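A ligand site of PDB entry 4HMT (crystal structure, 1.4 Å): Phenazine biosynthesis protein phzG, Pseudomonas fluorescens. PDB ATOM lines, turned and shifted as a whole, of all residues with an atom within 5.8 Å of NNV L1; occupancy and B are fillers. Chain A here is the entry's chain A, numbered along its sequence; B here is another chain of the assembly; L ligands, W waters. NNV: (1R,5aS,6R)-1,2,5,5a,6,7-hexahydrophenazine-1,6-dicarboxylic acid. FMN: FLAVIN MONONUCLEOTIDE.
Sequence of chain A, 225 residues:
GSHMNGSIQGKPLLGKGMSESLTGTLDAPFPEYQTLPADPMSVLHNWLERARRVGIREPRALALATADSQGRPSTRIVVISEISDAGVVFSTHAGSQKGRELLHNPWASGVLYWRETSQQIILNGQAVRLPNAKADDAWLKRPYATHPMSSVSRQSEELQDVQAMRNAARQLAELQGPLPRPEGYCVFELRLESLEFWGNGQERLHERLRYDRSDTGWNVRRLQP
An oxygen (O19) of NNV L1 is in hydrogen-bond range of the side-chain hydroxyl (OG) of Ser 21 of chain B, at 2.8 Å. O3' of FMN L2 sits at hydrogen-bond distance from NE1 of Trp 198 of chain B (3.4 Å). The backbone NH (N) of Val 79 sits at hydrogen-bond distance from an oxygen (O4) of FMN L2 (3.0 Å). A nitrogen (N3) of FMN L2 lies within hydrogen-bond range of the backbone carbonyl oxygen (O) of Ser 91. The backbone NH (N) of Ser 21 of chain B is in hydrogen-bond range of an oxygen (O19) of NNV L1 (2.8 Å). The side-chain hydroxyl (OG) of Ser 150 is in hydrogen-bond range of an oxygen (O13) of NNV L1. The side-chain hydroxyl of Thr 92 lies within hydrogen-bond range of an oxygen (O2) of FMN L2. NE2 of His 93 is in hydrogen-bond range of O13 of NNV L1, at 2.7 Å. An oxygen (O2) of FMN L2 sits at hydrogen-bond distance from the side-chain amide nitrogen (NE2) of Gln 155. The guanidinium group (NH1) of Arg 142 lies within salt-bridge range of an oxygen (O20) of NNV L1, 2.8 Å away.
OG of Ser 150 lies within hydrogen-bond range of O of Thr 146 (3.2 Å). The backbone NH (N) of His 93 is in hydrogen-bond range of the side-chain amide oxygen (OE1) of Gln 155, 3.5 Å away.
Merely in contact with NNV L1: Tyr 185 (3.5 Å), Ser 91 (3.6 Å), His 206 of chain B (3.6 Å), Val 79 (3.8 Å), Glu 20 of chain B (3.8 Å) and Leu 22 of chain B (3.9 Å). Hydrophobic or aromatic side chains within 4 Å of NNV L1: Val 79, His 93, Tyr 185, Leu 22 of chain B and His 206 of chain B. Within 4 Å of NNV L1: Val 79, Ser 91, His 93, Arg 142, Ser 150, Tyr 185, Glu 20 of chain B, Ser 21 of chain B, Leu 22 of chain B and His 206 of chain B. The nearest printed residue that does not touch NNV L1 is Thr 92 (4.02 Å).
Water W7 bridges N17 of NNV L1 (2.9 Å) and O of Pro 225 of chain B (2.9 Å). Water W2 bridges the backbone carbonyl oxygen (O) of Ser 19 of chain B (2.8 Å) and an oxygen (O19) of NNV L1 (2.9 Å). Water W5 lies within hydrogen-bond range of the chain-end carboxylate of Pro 225 of chain B, an oxygen (O13) of NNV L1 and a ring nitrogen (NE2) of His 93. Water W4 bridges O14 of NNV L1 (3.0 Å) and NE2 of His 206 of chain B (3.5 Å). Water W1 lies within hydrogen-bond range of O of Thr 146 (3.0 Å), OG of Ser 150 (3.0 Å) and O14 of NNV L1 (3.1 Å). Water W6 lies within hydrogen-bond range of OG of Ser 150 (2.8 Å), NE of Arg 142 (2.9 Å), OG1 of Thr 146 (3.0 Å) and O14 of NNV L1 (3.4 Å).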
ATOM      1  N   VAL A  79      -0.486  30.530  -6.791  1.00  0.00           N
ATOM      2  CA  VAL A  79      -0.377  30.580  -5.329  1.00  0.00           C
ATOM      3  C   VAL A  79      -0.687  31.964  -4.797  1.00  0.00           C
ATOM      4  O   VAL A  79      -0.128  32.969  -5.243  1.00  0.00           O
ATOM      5  CB  VAL A  79       1.039  30.191  -4.857  1.00  0.00           C
ATOM      6  CG1 VAL A  79       1.132  30.242  -3.348  1.00  0.00           C
ATOM      7  CG2 VAL A  79       1.412  28.827  -5.348  1.00  0.00           C
ATOM      8  N   SER A  91       1.535  36.481  -8.004  1.00  0.00           N
ATOM      9  CA  SER A  91       2.447  36.904  -9.039  1.00  0.00           C
ATOM     10  C   SER A  91       2.330  36.021 -10.259  1.00  0.00           C
ATOM     11  O   SER A  91       1.966  34.839 -10.143  1.00  0.00           O
ATOM     12  CB  SER A  91       3.904  36.787  -8.534  1.00  0.00           C
ATOM     13  OG  SER A  91       4.146  37.711  -7.496  1.00  0.00           O
ATOM     14  N   THR A  92       2.660  36.568 -11.420  1.00  0.00           N
ATOM     15  CA  THR A  92       2.598  35.822 -12.650  1.00  0.00           C
ATOM     16  C   THR A  92       3.396  36.596 -13.716  1.00  0.00           C
ATOM     17  O   THR A  92       4.119  37.523 -13.392  1.00  0.00           O
ATOM     18  CB  THR A  92       1.155  35.585 -13.104  1.00  0.00           C
ATOM     19  OG1 THR A  92       1.139  34.565 -14.106  1.00  0.00           O
ATOM     20  CG2 THR A  92       0.480  36.743 -13.587  1.00  0.00           C
ATOM     21  N   HIS A  93       3.319  36.154 -14.966  1.00  0.00           N
ATOM     22  CA  HIS A  93       3.863  36.904 -16.070  1.00  0.00           C
ATOM     23  C   HIS A  93       2.800  37.600 -16.872  1.00  0.00           C
ATOM     24  O   HIS A  93       1.740  37.028 -17.186  1.00  0.00           O
ATOM     25  CB  HIS A  93       4.640  35.965 -16.959  1.00  0.00           C
ATOM     26  CG  HIS A  93       5.800  35.364 -16.256  1.00  0.00           C
ATOM     27  ND1 HIS A  93       7.092  35.836 -16.405  1.00  0.00           N
ATOM     28  CD2 HIS A  93       5.876  34.321 -15.407  1.00  0.00           C
ATOM     29  CE1 HIS A  93       7.898  35.114 -15.650  1.00  0.00           C
ATOM     30  NE2 HIS A  93       7.192  34.173 -15.056  1.00  0.00           N
ATOM     31  N   ARG A 142      11.323  35.699  -3.912  1.00  0.00           N
ATOM     32  CA  ARG A 142      11.332  34.348  -4.425  1.00  0.00           C
ATOM     33  C   ARG A 142      12.702  33.755  -4.187  1.00  0.00           C
ATOM     34  O   ARG A 142      13.747  34.448  -4.231  1.00  0.00           O
ATOM     35  CB  ARG A 142      11.104  34.333  -5.965  1.00  0.00           C
ATOM     36  CG  ARG A 142       9.799  34.894  -6.449  1.00  0.00           C
ATOM     37  CD  ARG A 142       8.689  33.810  -6.419  1.00  0.00           C
ATOM     38  NE  ARG A 142       8.818  32.837  -7.504  1.00  0.00           N
ATOM     39  CZ  ARG A 142       8.370  31.584  -7.457  1.00  0.00           C
ATOM     40  NH1 ARG A 142       7.848  31.028  -6.332  1.00  0.00           N
ATOM     41  NH2 ARG A 142       8.478  30.846  -8.526  1.00  0.00           N
ATOM     42  N   THR A 146      14.750  30.007  -8.410  1.00  0.00           N
ATOM     43  CA  THR A 146      13.676  30.196  -9.368  1.00  0.00           C
ATOM     44  C   THR A 146      13.980  31.234 -10.434  1.00  0.00           C
ATOM     45  O   THR A 146      13.295  31.321 -11.477  1.00  0.00           O
ATOM     46  CB  THR A 146      12.332  30.621  -8.693  1.00  0.00           C
ATOM     47  OG1 THR A 146      12.403  31.950  -8.178  1.00  0.00           O
ATOM     48  CG2 THR A 146      11.937  29.687  -7.610  1.00  0.00           C
ATOM     49  N   MET A 149      14.861  30.173 -14.581  1.00  0.00           N
ATOM     50  CA  MET A 149      13.848  29.760 -15.499  1.00  0.00           C
ATOM     51  C   MET A 149      12.855  30.891 -15.725  1.00  0.00           C
ATOM     52  O   MET A 149      12.332  31.049 -16.850  1.00  0.00           O
ATOM     53  CB  MET A 149      13.150  28.479 -14.992  1.00  0.00           C
ATOM     54  CG  MET A 149      12.253  27.817 -16.067  1.00  0.00           C
ATOM     55  SD  MET A 149      13.259  27.303 -17.526  1.00  0.00           S
ATOM     56  CE  MET A 149      14.332  26.096 -16.780  1.00  0.00           C
ATOM     57  N   SER A 150      12.520  31.626 -14.663  1.00  0.00           N
ATOM     58  CA  SER A 150      11.559  32.721 -14.817  1.00  0.00           C
ATOM     59  C   SER A 150      12.073  33.817 -15.733  1.00  0.00           C
ATOM     60  O   SER A 150      11.296  34.577 -16.314  1.00  0.00           O
ATOM     61  CB  SER A 150      11.172  33.331 -13.473  1.00  0.00           C
ATOM     62  OG  SER A 150      10.527  32.399 -12.655  1.00  0.00           O
ATOM     63  N   GLN A 155       6.343  32.913 -20.437  1.00  0.00           N
ATOM     64  CA  GLN A 155       5.268  32.032 -19.979  1.00  0.00           C
ATOM     65  C   GLN A 155       4.097  31.948 -20.944  1.00  0.00           C
ATOM     66  O   GLN A 155       3.555  32.955 -21.311  1.00  0.00           O
ATOM     67  CB  GLN A 155       4.806  32.482 -18.604  1.00  0.00           C
ATOM     68  CG  GLN A 155       3.830  31.527 -17.928  1.00  0.00           C
ATOM     69  CD  GLN A 155       3.450  32.037 -16.557  1.00  0.00           C
ATOM     70  OE1 GLN A 155       2.788  33.061 -16.437  1.00  0.00           O
ATOM     71  NE2 GLN A 155       3.856  31.317 -15.484  1.00  0.00           N
ATOM     72  N   TYR A 185       7.449  40.087 -15.300  1.00  0.00           N
ATOM     73  CA  TYR A 185       7.109  39.525 -13.985  1.00  0.00           C
ATOM     74  C   TYR A 185       6.319  40.562 -13.205  1.00  0.00           C
ATOM     75  O   TYR A 185       6.834  41.651 -12.923  1.00  0.00           O
ATOM     76  CB  TYR A 185       8.358  39.159 -13.224  1.00  0.00           C
ATOM     77  CG  TYR A 185       8.088  38.301 -12.011  1.00  0.00           C
ATOM     78  CD1 TYR A 185       7.837  38.871 -10.763  1.00  0.00           C
ATOM     79  CD2 TYR A 185       8.099  36.915 -12.117  1.00  0.00           C
ATOM     80  CE1 TYR A 185       7.579  38.045  -9.655  1.00  0.00           C
ATOM     81  CE2 TYR A 185       7.878  36.097 -11.021  1.00  0.00           C
ATOM     82  CZ  TYR A 185       7.587  36.664  -9.802  1.00  0.00           C
ATOM     83  OH  TYR A 185       7.371  35.783  -8.728  1.00  0.00           O
ATOM     84  N   SER B  19       9.494  30.605  -0.067  1.00  0.00           N
ATOM     85  CA  SER B  19       9.595  29.167  -0.358  1.00  0.00           C
ATOM     86  C   SER B  19       8.701  28.817  -1.524  1.00  0.00           C
ATOM     87  O   SER B  19       7.578  29.357  -1.665  1.00  0.00           O
ATOM     88  CB  SER B  19       9.174  28.326   0.864  1.00  0.00           C
ATOM     89  N   GLU B  20       9.157  27.869  -2.349  1.00  0.00           N
ATOM     90  CA  GLU B  20       8.297  27.351  -3.419  1.00  0.00           C
ATOM     91  C   GLU B  20       7.237  26.500  -2.738  1.00  0.00           C
ATOM     92  O   GLU B  20       7.465  25.923  -1.660  1.00  0.00           O
ATOM     93  CB  GLU B  20       9.099  26.555  -4.469  1.00  0.00           C
ATOM     94  CG  GLU B  20      10.248  27.398  -5.048  1.00  0.00           C
ATOM     95  CD  GLU B  20      11.259  26.550  -5.822  1.00  0.00           C
ATOM     96  OE1 GLU B  20      10.941  26.081  -6.975  1.00  0.00           O
ATOM     97  OE2 GLU B  20      12.378  26.377  -5.271  1.00  0.00           O
ATOM     98  N   SER B  21       6.072  26.408  -3.332  1.00  0.00           N
ATOM     99  CA  SER B  21       4.953  25.851  -2.583  1.00  0.00           C
ATOM    100  C   SER B  21       4.654  24.411  -2.947  1.00  0.00           C
ATOM    101  O   SER B  21       3.900  23.774  -2.215  1.00  0.00           O
ATOM    102  CB  SER B  21       3.707  26.697  -2.777  1.00  0.00           C
ATOM    103  OG  SER B  21       3.172  26.480  -4.072  1.00  0.00           O
ATOM    104  N   LEU B  22       5.271  23.869  -4.011  1.00  0.00           N
ATOM    105  CA  LEU B  22       4.964  22.487  -4.395  1.00  0.00           C
ATOM    106  C   LEU B  22       5.417  21.507  -3.340  1.00  0.00           C
ATOM    107  O   LEU B  22       6.555  21.622  -2.848  1.00  0.00           O
ATOM    108  CB  LEU B  22       5.621  22.081  -5.708  1.00  0.00           C
ATOM    109  CG  LEU B  22       5.216  22.934  -6.891  1.00  0.00           C
ATOM    110  CD1 LEU B  22       6.039  22.496  -8.110  1.00  0.00           C
ATOM    111  CD2 LEU B  22       3.753  22.802  -7.210  1.00  0.00           C
ATOM    112  N   TRP B 198       0.060  19.528 -17.364  1.00  0.00           N
ATOM    113  CA  TRP B 198       1.168  20.202 -16.713  1.00  0.00           C
ATOM    114  C   TRP B 198       1.835  19.254 -15.737  1.00  0.00           C
ATOM    115  O   TRP B 198       1.185  18.705 -14.831  1.00  0.00           O
ATOM    116  CB  TRP B 198       0.611  21.406 -15.969  1.00  0.00           C
ATOM    117  CG  TRP B 198       1.616  22.384 -15.345  1.00  0.00           C
ATOM    118  CD1 TRP B 198       1.922  23.602 -15.841  1.00  0.00           C
ATOM    119  CD2 TRP B 198       2.399  22.236 -14.139  1.00  0.00           C
ATOM    120  NE1 TRP B 198       2.814  24.251 -15.049  1.00  0.00           N
ATOM    121  CE2 TRP B 198       3.129  23.435 -13.984  1.00  0.00           C
ATOM    122  CE3 TRP B 198       2.512  21.238 -13.151  1.00  0.00           C
ATOM    123  CZ2 TRP B 198       3.984  23.639 -12.928  1.00  0.00           C
ATOM    124  CZ3 TRP B 198       3.384  21.456 -12.102  1.00  0.00           C
ATOM    125  CH2 TRP B 198       4.097  22.656 -11.995  1.00  0.00           C
ATOM    126  N   HIS B 206       9.021  23.373 -16.124  1.00  0.00           N
ATOM    127  CA  HIS B 206       7.740  22.683 -16.011  1.00  0.00           C
ATOM    128  C   HIS B 206       7.232  22.315 -17.414  1.00  0.00           C
ATOM    129  O   HIS B 206       7.440  23.041 -18.382  1.00  0.00           O
ATOM    130  CB  HIS B 206       6.729  23.534 -15.301  1.00  0.00           C
ATOM    131  CG  HIS B 206       7.204  24.105 -14.033  1.00  0.00           C
ATOM    132  ND1 HIS B 206       7.754  23.316 -13.052  1.00  0.00           N
ATOM    133  CD2 HIS B 206       7.209  25.372 -13.561  1.00  0.00           C
ATOM    134  CE1 HIS B 206       8.116  24.091 -12.032  1.00  0.00           C
ATOM    135  NE2 HIS B 206       7.812  25.349 -12.336  1.00  0.00           N
ATOM    136  N   PRO B 225       7.084  27.470 -19.546  1.00  0.00           N
ATOM    137  CA  PRO B 225       6.570  27.460 -18.187  1.00  0.00           C
ATOM    138  C   PRO B 225       6.333  28.782 -17.538  1.00  0.00           C
ATOM    139  O   PRO B 225       5.492  28.830 -16.612  1.00  0.00           O
ATOM    140  CB  PRO B 225       7.654  26.703 -17.422  1.00  0.00           C
ATOM    141  CG  PRO B 225       8.842  26.840 -18.188  1.00  0.00           C
ATOM    142  CD  PRO B 225       8.440  26.939 -19.634  1.00  0.00           C
ATOM    143  OXT PRO B 225       6.955  29.793 -17.887  1.00  0.00           O
HETATM  144  C01 NNV L   1       4.823  26.118  -9.613  1.00  0.00           C
HETATM  145  C02 NNV L   1       4.580  26.497  -8.236  1.00  0.00           C
HETATM  146  C03 NNV L   1       4.669  27.955  -7.813  1.00  0.00           C
HETATM  147  C04 NNV L   1       4.978  28.896  -8.926  1.00  0.00           C
HETATM  148  N05 NNV L   1       4.957  30.300  -8.641  1.00  0.00           N
HETATM  149  C06 NNV L   1       5.190  31.241  -9.689  1.00  0.00           C
HETATM  150  C07 NNV L   1       5.190  32.666  -9.361  1.00  0.00           C
HETATM  151  C08 NNV L   1       5.323  33.596 -10.462  1.00  0.00           C
HETATM  152  C09 NNV L   1       5.502  33.171 -11.834  1.00  0.00           C
HETATM  153  C10 NNV L   1       5.517  30.798 -10.983  1.00  0.00           C
HETATM  154  C11 NNV L   1       5.910  31.764 -12.051  1.00  0.00           C
HETATM  155  C12 NNV L   1       7.449  31.664 -12.294  1.00  0.00           C
HETATM  156  O13 NNV L   1       7.977  32.210 -13.344  1.00  0.00           O
HETATM  157  O14 NNV L   1       8.263  31.017 -11.533  1.00  0.00           O
HETATM  158  C15 NNV L   1       5.139  28.508 -10.298  1.00  0.00           C
HETATM  159  C16 NNV L   1       5.065  27.067 -10.696  1.00  0.00           C
HETATM  160  N17 NNV L   1       5.365  29.448 -11.238  1.00  0.00           N
HETATM  161  C18 NNV L   1       5.583  28.155  -6.647  1.00  0.00           C
HETATM  162  O19 NNV L   1       5.044  27.895  -5.520  1.00  0.00           O
HETATM  163  O20 NNV L   1       6.807  28.493  -6.825  1.00  0.00           O
HETATM  164  N1  FMN L   2       2.033  30.316 -12.339  1.00  0.00           N
HETATM  165  C2  FMN L   2       2.146  31.628 -12.065  1.00  0.00           C
HETATM  166  O2  FMN L   2       2.343  32.462 -12.966  1.00  0.00           O
HETATM  167  N3  FMN L   2       2.001  32.084 -10.763  1.00  0.00           N
HETATM  168  C4  FMN L   2       1.840  31.247  -9.692  1.00  0.00           C
HETATM  169  O4  FMN L   2       1.669  31.708  -8.563  1.00  0.00           O
HETATM  170  C4A FMN L   2       1.764  29.891  -9.979  1.00  0.00           C
HETATM  171  N5  FMN L   2       1.598  28.972  -8.975  1.00  0.00           N
HETATM  172  C5A FMN L   2       1.433  27.662  -9.308  1.00  0.00           C
HETATM  173  C6  FMN L   2       1.155  26.717  -8.299  1.00  0.00           C
HETATM  174  C7  FMN L   2       0.969  25.361  -8.532  1.00  0.00           C
HETATM  175  C7M FMN L   2       0.672  24.450  -7.365  1.00  0.00           C
HETATM  176  C8  FMN L   2       1.068  24.892  -9.850  1.00  0.00           C
HETATM  177  C8M FMN L   2       0.900  23.461 -10.233  1.00  0.00           C
HETATM  178  C9  FMN L   2       1.317  25.820 -10.858  1.00  0.00           C
HETATM  179  C9A FMN L   2       1.526  27.192 -10.613  1.00  0.00           C
HETATM  180  N10 FMN L   2       1.760  28.126 -11.629  1.00  0.00           N
HETATM  181  C10 FMN L   2       1.842  29.457 -11.308  1.00  0.00           C
HETATM  182  C1' FMN L   2       1.758  27.731 -13.079  1.00  0.00           C
HETATM  183  C2' FMN L   2       0.322  27.975 -13.603  1.00  0.00           C
HETATM  184  O2' FMN L   2      -0.575  26.928 -13.166  1.00  0.00           O
HETATM  185  C3' FMN L   2       0.270  28.078 -15.121  1.00  0.00           C
HETATM  186  O3' FMN L   2       0.901  26.946 -15.762  1.00  0.00           O
HETATM  187  C4' FMN L   2       0.943  29.355 -15.608  1.00  0.00           C
HETATM  188  O4' FMN L   2       0.773  30.461 -14.727  1.00  0.00           O
HETATM  189  C5' FMN L   2       0.453  29.730 -16.985  1.00  0.00           C
HETATM  190  O5' FMN L   2      -0.964  29.883 -16.990  1.00  0.00           O
HETATM  191  P   FMN L   2      -1.719  30.543 -18.214  1.00  0.00           P
HETATM  192  O1P FMN L   2      -1.612  32.068 -18.053  1.00  0.00           O
HETATM  193  O2P FMN L   2      -1.085  30.013 -19.477  1.00  0.00           O
HETATM  194  O3P FMN L   2      -3.149  30.065 -18.098  1.00  0.00           O
HETATM  195  O   HOH W   1      10.982  29.515 -11.861  1.00  0.00           O
HETATM  196  O   HOH W   2       5.685  29.951  -3.581  1.00  0.00           O
HETATM  197  O   HOH W   3       4.918  31.401  -6.008  1.00  0.00           O
HETATM  198  O   HOH W   4       9.085  28.232 -10.928  1.00  0.00           O
HETATM  199  O   HOH W   5       8.067  31.499 -16.202  1.00  0.00           O
HETATM  200  O   HOH W   6      10.366  33.238  -9.970  1.00  0.00           O
HETATM  201  O   HOH W   7       6.285  28.536 -13.815  1.00  0.00           O
